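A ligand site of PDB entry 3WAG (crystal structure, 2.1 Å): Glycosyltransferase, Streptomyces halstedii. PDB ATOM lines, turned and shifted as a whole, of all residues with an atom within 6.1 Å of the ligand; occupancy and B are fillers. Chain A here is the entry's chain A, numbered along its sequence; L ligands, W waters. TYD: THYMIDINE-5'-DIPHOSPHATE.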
ATOM      1  N   SER A  12       1.469   7.265  16.158  1.00  0.00           N
ATOM      2  CA  SER A  12       0.809   7.677  17.354  1.00  0.00           C
ATOM      3  C   SER A  12      -0.688   7.254  17.302  1.00  0.00           C
ATOM      4  O   SER A  12      -1.192   6.742  18.279  1.00  0.00           O
ATOM      5  CB  SER A  12       0.984   9.217  17.539  1.00  0.00           C
ATOM      6  OG  SER A  12       0.346   9.675  18.722  1.00  0.00           O
ATOM      7  N   TYR A  15      -0.731   3.474  17.662  1.00  0.00           N
ATOM      8  CA  TYR A  15      -0.479   3.057  19.041  1.00  0.00           C
ATOM      9  C   TYR A  15      -1.741   3.202  19.905  1.00  0.00           C
ATOM     10  O   TYR A  15      -1.975   2.391  20.766  1.00  0.00           O
ATOM     11  CB  TYR A  15       0.620   3.921  19.644  1.00  0.00           C
ATOM     12  CG  TYR A  15       1.998   3.631  19.154  1.00  0.00           C
ATOM     13  CD1 TYR A  15       2.248   2.590  18.242  1.00  0.00           C
ATOM     14  CD2 TYR A  15       3.061   4.421  19.618  1.00  0.00           C
ATOM     15  CE1 TYR A  15       3.527   2.324  17.840  1.00  0.00           C
ATOM     16  CE2 TYR A  15       4.350   4.157  19.247  1.00  0.00           C
ATOM     17  CZ  TYR A  15       4.569   3.114  18.340  1.00  0.00           C
ATOM     18  OH  TYR A  15       5.835   2.878  17.924  1.00  0.00           O
ATOM     19  N   PRO A 228      -2.264   3.177  27.319  1.00  0.00           N
ATOM     20  CA  PRO A 228      -1.512   3.998  26.366  1.00  0.00           C
ATOM     21  C   PRO A 228      -0.354   3.126  25.872  1.00  0.00           C
ATOM     22  O   PRO A 228       0.481   2.794  26.667  1.00  0.00           O
ATOM     23  CB  PRO A 228      -0.970   5.173  27.241  1.00  0.00           C
ATOM     24  CG  PRO A 228      -0.915   4.619  28.664  1.00  0.00           C
ATOM     25  CD  PRO A 228      -1.739   3.306  28.702  1.00  0.00           C
ATOM     26  N   PHE A 229      -0.277   2.767  24.596  1.00  0.00           N
ATOM     27  CA  PHE A 229       0.794   1.833  24.164  1.00  0.00           C
ATOM     28  C   PHE A 229       1.936   2.683  23.672  1.00  0.00           C
ATOM     29  O   PHE A 229       1.733   3.606  22.889  1.00  0.00           O
ATOM     30  CB  PHE A 229       0.309   0.974  23.014  1.00  0.00           C
ATOM     31  CG  PHE A 229       1.385   0.052  22.408  1.00  0.00           C
ATOM     32  CD1 PHE A 229       1.860  -1.073  23.105  1.00  0.00           C
ATOM     33  CD2 PHE A 229       1.904   0.343  21.124  1.00  0.00           C
ATOM     34  CE1 PHE A 229       2.798  -1.926  22.479  1.00  0.00           C
ATOM     35  CE2 PHE A 229       2.846  -0.492  20.511  1.00  0.00           C
ATOM     36  CZ  PHE A 229       3.266  -1.632  21.177  1.00  0.00           C
ATOM     37  N   ASN A 230       3.106   2.405  24.194  1.00  0.00           N
ATOM     38  CA  ASN A 230       4.248   3.311  23.988  1.00  0.00           C
ATOM     39  C   ASN A 230       5.261   2.839  22.908  1.00  0.00           C
ATOM     40  O   ASN A 230       6.389   3.308  22.897  1.00  0.00           O
ATOM     41  CB  ASN A 230       4.960   3.538  25.315  1.00  0.00           C
ATOM     42  CG  ASN A 230       4.091   4.271  26.341  1.00  0.00           C
ATOM     43  OD1 ASN A 230       3.374   5.220  26.013  1.00  0.00           O
ATOM     44  ND2 ASN A 230       4.128   3.803  27.566  1.00  0.00           N
ATOM     45  N   GLY A 231       4.856   1.897  22.037  1.00  0.00           N
ATOM     46  CA  GLY A 231       5.704   1.331  20.987  1.00  0.00           C
ATOM     47  C   GLY A 231       6.767   0.383  21.548  1.00  0.00           C
ATOM     48  O   GLY A 231       6.641  -0.038  22.698  1.00  0.00           O
ATOM     49  N   THR A 251      10.142  15.346  28.661  1.00  0.00           N
ATOM     50  CA  THR A 251       9.983  15.024  27.235  1.00  0.00           C
ATOM     51  C   THR A 251       9.423  16.220  26.500  1.00  0.00           C
ATOM     52  O   THR A 251       8.211  16.293  26.229  1.00  0.00           O
ATOM     53  CB  THR A 251       9.067  13.820  26.949  1.00  0.00           C
ATOM     54  OG1 THR A 251       7.931  13.893  27.780  1.00  0.00           O
ATOM     55  CG2 THR A 251       9.728  12.590  27.265  1.00  0.00           C
ATOM     56  N   THR A 283      14.413  13.112  27.245  1.00  0.00           N
ATOM     57  CA  THR A 283      14.523  12.626  25.895  1.00  0.00           C
ATOM     58  C   THR A 283      15.031  13.766  24.977  1.00  0.00           C
ATOM     59  O   THR A 283      14.447  14.859  24.922  1.00  0.00           O
ATOM     60  CB  THR A 283      13.179  12.082  25.394  1.00  0.00           C
ATOM     61  OG1 THR A 283      12.203  13.135  25.522  1.00  0.00           O
ATOM     62  CG2 THR A 283      12.727  10.863  26.210  1.00  0.00           C
ATOM     63  N   ASP A 303      17.668   8.849  23.956  1.00  0.00           N
ATOM     64  CA  ASP A 303      16.765   9.044  22.776  1.00  0.00           C
ATOM     65  C   ASP A 303      15.279   8.821  23.094  1.00  0.00           C
ATOM     66  O   ASP A 303      14.415   9.386  22.422  1.00  0.00           O
ATOM     67  CB  ASP A 303      17.044   8.069  21.627  1.00  0.00           C
ATOM     68  CG  ASP A 303      18.478   7.817  21.414  1.00  0.00           C
ATOM     69  OD1 ASP A 303      19.155   8.690  20.813  1.00  0.00           O
ATOM     70  OD2 ASP A 303      18.916   6.737  21.847  1.00  0.00           O
ATOM     71  N   PHE A 304      15.001   7.916  24.040  1.00  0.00           N
ATOM     72  CA  PHE A 304      13.655   7.361  24.250  1.00  0.00           C
ATOM     73  C   PHE A 304      13.772   6.493  25.496  1.00  0.00           C
ATOM     74  O   PHE A 304      14.776   5.793  25.661  1.00  0.00           O
ATOM     75  CB  PHE A 304      13.226   6.470  23.065  1.00  0.00           C
ATOM     76  CG  PHE A 304      11.881   5.791  23.258  1.00  0.00           C
ATOM     77  CD1 PHE A 304      11.796   4.509  23.901  1.00  0.00           C
ATOM     78  CD2 PHE A 304      10.677   6.413  22.828  1.00  0.00           C
ATOM     79  CE1 PHE A 304      10.549   3.898  24.095  1.00  0.00           C
ATOM     80  CE2 PHE A 304       9.427   5.785  23.031  1.00  0.00           C
ATOM     81  CZ  PHE A 304       9.369   4.529  23.646  1.00  0.00           C
ATOM     82  N   VAL A 305      12.777   6.556  26.373  1.00  0.00           N
ATOM     83  CA  VAL A 305      12.670   5.602  27.483  1.00  0.00           C
ATOM     84  C   VAL A 305      11.177   5.247  27.587  1.00  0.00           C
ATOM     85  O   VAL A 305      10.321   6.147  27.566  1.00  0.00           O
ATOM     86  CB  VAL A 305      13.267   6.206  28.792  1.00  0.00           C
ATOM     87  CG1 VAL A 305      12.855   7.654  28.970  1.00  0.00           C
ATOM     88  CG2 VAL A 305      13.016   5.346  30.016  1.00  0.00           C
ATOM     89  N   PRO A 306      10.861   3.952  27.654  1.00  0.00           N
ATOM     90  CA  PRO A 306       9.414   3.655  27.669  1.00  0.00           C
ATOM     91  C   PRO A 306       8.822   4.272  28.937  1.00  0.00           C
ATOM     92  O   PRO A 306       9.358   4.086  30.050  1.00  0.00           O
ATOM     93  CB  PRO A 306       9.326   2.109  27.714  1.00  0.00           C
ATOM     94  CG  PRO A 306      10.709   1.628  28.012  1.00  0.00           C
ATOM     95  CD  PRO A 306      11.705   2.747  27.794  1.00  0.00           C
ATOM     96  N   LEU A 307       7.717   4.982  28.788  1.00  0.00           N
ATOM     97  CA  LEU A 307       7.266   5.833  29.859  1.00  0.00           C
ATOM     98  C   LEU A 307       6.721   4.987  31.017  1.00  0.00           C
ATOM     99  O   LEU A 307       6.863   5.352  32.165  1.00  0.00           O
ATOM    100  CB  LEU A 307       6.225   6.742  29.259  1.00  0.00           C
ATOM    101  CG  LEU A 307       6.394   8.251  29.381  1.00  0.00           C
ATOM    102  CD1 LEU A 307       7.733   8.778  29.913  1.00  0.00           C
ATOM    103  CD2 LEU A 307       6.019   8.849  28.071  1.00  0.00           C
ATOM    104  N   HIS A 308       6.135   3.832  30.695  1.00  0.00           N
ATOM    105  CA  HIS A 308       5.580   2.887  31.678  1.00  0.00           C
ATOM    106  C   HIS A 308       6.616   2.283  32.576  1.00  0.00           C
ATOM    107  O   HIS A 308       6.281   1.842  33.635  1.00  0.00           O
ATOM    108  CB  HIS A 308       4.721   1.778  31.048  1.00  0.00           C
ATOM    109  CG  HIS A 308       5.428   1.051  29.935  1.00  0.00           C
ATOM    110  ND1 HIS A 308       5.912  -0.202  30.079  1.00  0.00           N
ATOM    111  CD2 HIS A 308       5.727   1.454  28.630  1.00  0.00           C
ATOM    112  CE1 HIS A 308       6.463  -0.594  28.894  1.00  0.00           C
ATOM    113  NE2 HIS A 308       6.320   0.402  28.014  1.00  0.00           N
ATOM    114  N   HIS A 319       5.913  17.882  29.924  1.00  0.00           N
ATOM    115  CA  HIS A 319       5.728  17.452  28.565  1.00  0.00           C
ATOM    116  C   HIS A 319       4.829  18.388  27.836  1.00  0.00           C
ATOM    117  O   HIS A 319       4.418  19.424  28.419  1.00  0.00           O
ATOM    118  CB  HIS A 319       5.228  15.980  28.514  1.00  0.00           C
ATOM    119  CG  HIS A 319       3.808  15.784  29.025  1.00  0.00           C
ATOM    120  ND1 HIS A 319       3.500  15.737  30.346  1.00  0.00           N
ATOM    121  CD2 HIS A 319       2.617  15.617  28.345  1.00  0.00           C
ATOM    122  CE1 HIS A 319       2.173  15.564  30.500  1.00  0.00           C
ATOM    123  NE2 HIS A 319       1.634  15.470  29.291  1.00  0.00           N
ATOM    124  N   HIS A 320       4.507  18.036  26.586  1.00  0.00           N
ATOM    125  CA  HIS A 320       3.675  18.854  25.663  1.00  0.00           C
ATOM    126  C   HIS A 320       2.177  18.652  25.770  1.00  0.00           C
ATOM    127  O   HIS A 320       1.388  19.271  25.018  1.00  0.00           O
ATOM    128  CB  HIS A 320       4.085  18.587  24.207  1.00  0.00           C
ATOM    129  CG  HIS A 320       4.174  17.117  23.927  1.00  0.00           C
ATOM    130  ND1 HIS A 320       5.279  16.376  24.259  1.00  0.00           N
ATOM    131  CD2 HIS A 320       3.222  16.233  23.465  1.00  0.00           C
ATOM    132  CE1 HIS A 320       5.039  15.080  23.960  1.00  0.00           C
ATOM    133  NE2 HIS A 320       3.782  14.993  23.471  1.00  0.00           N
ATOM    134  N   GLY A 321       1.736  17.794  26.665  1.00  0.00           N
ATOM    135  CA  GLY A 321       0.279  17.683  26.880  1.00  0.00           C
ATOM    136  C   GLY A 321      -0.442  16.706  25.969  1.00  0.00           C
ATOM    137  O   GLY A 321      -1.688  16.696  25.944  1.00  0.00           O
ATOM    138  N   GLY A 322       0.321  15.848  25.251  1.00  0.00           N
ATOM    139  CA  GLY A 322      -0.273  14.887  24.342  1.00  0.00           C
ATOM    140  C   GLY A 322      -0.997  13.732  25.042  1.00  0.00           C
ATOM    141  O   GLY A 322      -0.675  13.375  26.171  1.00  0.00           O
ATOM    142  N   GLY A 323      -1.951  13.127  24.341  1.00  0.00           N
ATOM    143  CA  GLY A 323      -2.737  12.000  24.821  1.00  0.00           C
ATOM    144  C   GLY A 323      -1.936  10.812  25.349  1.00  0.00           C
ATOM    145  O   GLY A 323      -2.299  10.249  26.382  1.00  0.00           O
ATOM    146  N   GLY A 324      -0.856  10.385  24.677  1.00  0.00           N
ATOM    147  CA  GLY A 324      -0.212   9.137  25.194  1.00  0.00           C
ATOM    148  C   GLY A 324       0.523   9.368  26.472  1.00  0.00           C
ATOM    149  O   GLY A 324       0.431   8.603  27.487  1.00  0.00           O
ATOM    150  N   THR A 325       1.307  10.428  26.462  1.00  0.00           N
ATOM    151  CA  THR A 325       2.084  10.828  27.619  1.00  0.00           C
ATOM    152  C   THR A 325       1.157  11.110  28.817  1.00  0.00           C
ATOM    153  O   THR A 325       1.457  10.662  29.937  1.00  0.00           O
ATOM    154  CB  THR A 325       2.894  12.106  27.263  1.00  0.00           C
ATOM    155  OG1 THR A 325       3.713  11.807  26.116  1.00  0.00           O
ATOM    156  CG2 THR A 325       3.803  12.502  28.407  1.00  0.00           C
ATOM    157  N   ARG A 326       0.061  11.851  28.597  1.00  0.00           N
ATOM    158  CA  ARG A 326      -0.762  12.264  29.720  1.00  0.00           C
ATOM    159  C   ARG A 326      -1.488  11.045  30.251  1.00  0.00           C
ATOM    160  O   ARG A 326      -1.595  10.882  31.463  1.00  0.00           O
ATOM    161  CB  ARG A 326      -1.714  13.393  29.383  1.00  0.00           C
ATOM    162  CG  ARG A 326      -2.914  13.002  28.534  1.00  0.00           C
ATOM    163  CD  ARG A 326      -3.459  14.222  27.852  1.00  0.00           C
ATOM    164  NE  ARG A 326      -4.597  13.793  27.072  1.00  0.00           N
ATOM    165  CZ  ARG A 326      -5.065  14.447  26.046  1.00  0.00           C
ATOM    166  NH1 ARG A 326      -4.502  15.595  25.679  1.00  0.00           N
ATOM    167  NH2 ARG A 326      -6.117  13.957  25.410  1.00  0.00           N
ATOM    168  N   ASN A 328      -0.315   8.132  30.249  1.00  0.00           N
ATOM    169  CA  ASN A 328       0.722   7.486  31.112  1.00  0.00           C
ATOM    170  C   ASN A 328       0.771   8.169  32.539  1.00  0.00           C
ATOM    171  O   ASN A 328       0.860   7.480  33.609  1.00  0.00           O
ATOM    172  CB  ASN A 328       2.115   7.513  30.441  1.00  0.00           C
ATOM    173  CG  ASN A 328       2.344   6.371  29.413  1.00  0.00           C
ATOM    174  OD1 ASN A 328       2.725   5.267  29.797  1.00  0.00           O
ATOM    175  ND2 ASN A 328       2.127   6.638  28.116  1.00  0.00           N
ATOM    176  N   ASN A 341       1.148  22.089  23.583  1.00  0.00           N
ATOM    177  CA  ASN A 341       1.078  22.096  22.142  1.00  0.00           C
ATOM    178  C   ASN A 341      -0.049  22.809  21.412  1.00  0.00           C
ATOM    179  O   ASN A 341       0.179  23.316  20.320  1.00  0.00           O
ATOM    180  CB  ASN A 341       0.894  20.635  21.729  1.00  0.00           C
ATOM    181  CG  ASN A 341       1.941  20.183  20.770  1.00  0.00           C
ATOM    182  OD1 ASN A 341       2.054  18.988  20.498  1.00  0.00           O
ATOM    183  ND2 ASN A 341       2.726  21.126  20.246  1.00  0.00           N
ATOM    184  N   GLU A 346      -4.438  19.790  23.554  1.00  0.00           N
ATOM    185  CA  GLU A 346      -3.514  19.810  24.671  1.00  0.00           C
ATOM    186  C   GLU A 346      -3.810  20.927  25.639  1.00  0.00           C
ATOM    187  O   GLU A 346      -3.479  20.830  26.807  1.00  0.00           O
ATOM    188  CB  GLU A 346      -2.065  19.913  24.170  1.00  0.00           C
ATOM    189  CG  GLU A 346      -1.557  18.628  23.487  1.00  0.00           C
ATOM    190  CD  GLU A 346      -1.973  18.431  22.025  1.00  0.00           C
ATOM    191  OE1 GLU A 346      -2.846  19.182  21.463  1.00  0.00           O
ATOM    192  OE2 GLU A 346      -1.388  17.478  21.439  1.00  0.00           O
HETATM  193  PA  TYD L   1       3.820  10.740  21.156  1.00  0.00           P
HETATM  194  O1A TYD L   1       4.820  11.901  21.353  1.00  0.00           O
HETATM  195  O2A TYD L   1       2.999  10.625  19.885  1.00  0.00           O
HETATM  196  O3A TYD L   1       2.812  10.771  22.453  1.00  0.00           O
HETATM  197  PB  TYD L   1       1.688  11.905  22.736  1.00  0.00           P
HETATM  198  O1B TYD L   1       1.835  13.080  21.782  1.00  0.00           O
HETATM  199  O2B TYD L   1       2.122  12.217  24.139  1.00  0.00           O
HETATM  200  O3B TYD L   1       0.356  11.207  22.433  1.00  0.00           O
HETATM  201  O5' TYD L   1       4.444   9.271  21.527  1.00  0.00           O
HETATM  202  C5' TYD L   1       3.744   8.034  21.392  1.00  0.00           C
HETATM  203  C4' TYD L   1       3.820   7.262  22.717  1.00  0.00           C
HETATM  204  O4' TYD L   1       5.177   6.981  23.099  1.00  0.00           O
HETATM  205  C3' TYD L   1       3.161   7.983  23.907  1.00  0.00           C
HETATM  206  O3' TYD L   1       2.355   7.004  24.642  1.00  0.00           O
HETATM  207  C2' TYD L   1       4.338   8.494  24.755  1.00  0.00           C
HETATM  208  C1' TYD L   1       5.414   7.417  24.450  1.00  0.00           C
HETATM  209  N1  TYD L   1       6.808   7.805  24.630  1.00  0.00           N
HETATM  210  C2  TYD L   1       7.606   7.014  25.477  1.00  0.00           C
HETATM  211  O2  TYD L   1       7.122   5.995  26.041  1.00  0.00           O
HETATM  212  N3  TYD L   1       8.906   7.310  25.680  1.00  0.00           N
HETATM  213  C4  TYD L   1       9.531   8.355  25.099  1.00  0.00           C
HETATM  214  O4  TYD L   1      10.728   8.611  25.354  1.00  0.00           O
HETATM  215  C5  TYD L   1       8.743   9.231  24.198  1.00  0.00           C
HETATM  216  C5M TYD L   1       9.437  10.439  23.586  1.00  0.00           C
HETATM  217  C6  TYD L   1       7.371   8.893  24.013  1.00  0.00           C
HETATM  218  O   HOH W   1       0.449   6.121  23.402  1.00  0.00           O
HETATM  219  O   HOH W   2       1.265  16.053  21.513  1.00  0.00           O
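OD1 of Asn 230 is in hydrogen-bond range of ND2 of Asn 328, at 2.8 Å.
The backbone carbonyl oxygen (O) of Gly 324 lies within hydrogen-bond range of the side-chain amide nitrogen (ND2) of Asn 328, at 2.7 Å.
The backbone carbonyl oxygen of His 320 is in hydrogen-bond range of the backbone NH of Asn 341 (3.2 Å).
Phe 229 touches the ligand (O to O3', 3.9 Å).
Thr 283 touches the ligand (CG2 to O4, 3.1 Å).
Phe 304 touches the ligand.
CA of Pro 306 touches O2 of the ligand, at 3.7 Å.
Gly 322 touches the ligand (C to O2B, 3.6 Å).
Gly 323 touches the ligand (N to O3B, 3.6 Å).
ND2 of Asn 328 touches O3' of the ligand, at 3.5 Å.
Hydrophobic or aromatic side chains within 4 Å of the ligand: Phe 304, Leu 307 and His 320.
Of the 25 residues printed, 14 come within 4 Å of the ligand.
Along chain A the residues within 4 Å of the ligand span positions 12 to 328.
OD1 of Asn 230 sits at hydrogen-bond distance from O3' of the ligand (2.5 Å).
O2B of the ligand is in hydrogen-bond range of N of Thr 325, at 3.0 Å.
OG1 of Thr 325 lies within hydrogen-bond range of O2B of the ligand (2.6 Å).
An oxygen (O4) of the ligand lies within hydrogen-bond range of the backbone NH (N) of Val 305.
A nitrogen (N3) of the ligand lies within hydrogen-bond range of the backbone carbonyl oxygen (O) of Val 305.
N of Gly 324 lies within hydrogen-bond range of O3B of the ligand, at 2.7 Å.
The backbone NH (N) of Leu 307 is in hydrogen-bond range of an oxygen (O2) of the ligand, 3.0 Å away.
O2A of the ligand lies within hydrogen-bond range of OG of Ser 12 (3.0 Å).
A ring nitrogen (NE2) of His 320 lies within hydrogen-bond range of an oxygen (O1B) of the ligand, 3.2 Å away.
Water W1 bridges O3' of the ligand and O of Phe 229.
Water W2 lies within hydrogen-bond range of OE2 of Glu 346 (3.0 Å), O1B of the ligand (3.0 Å), OD1 of Asn 341 (3.2 Å) and NE2 of His 320 (3.4 Å).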
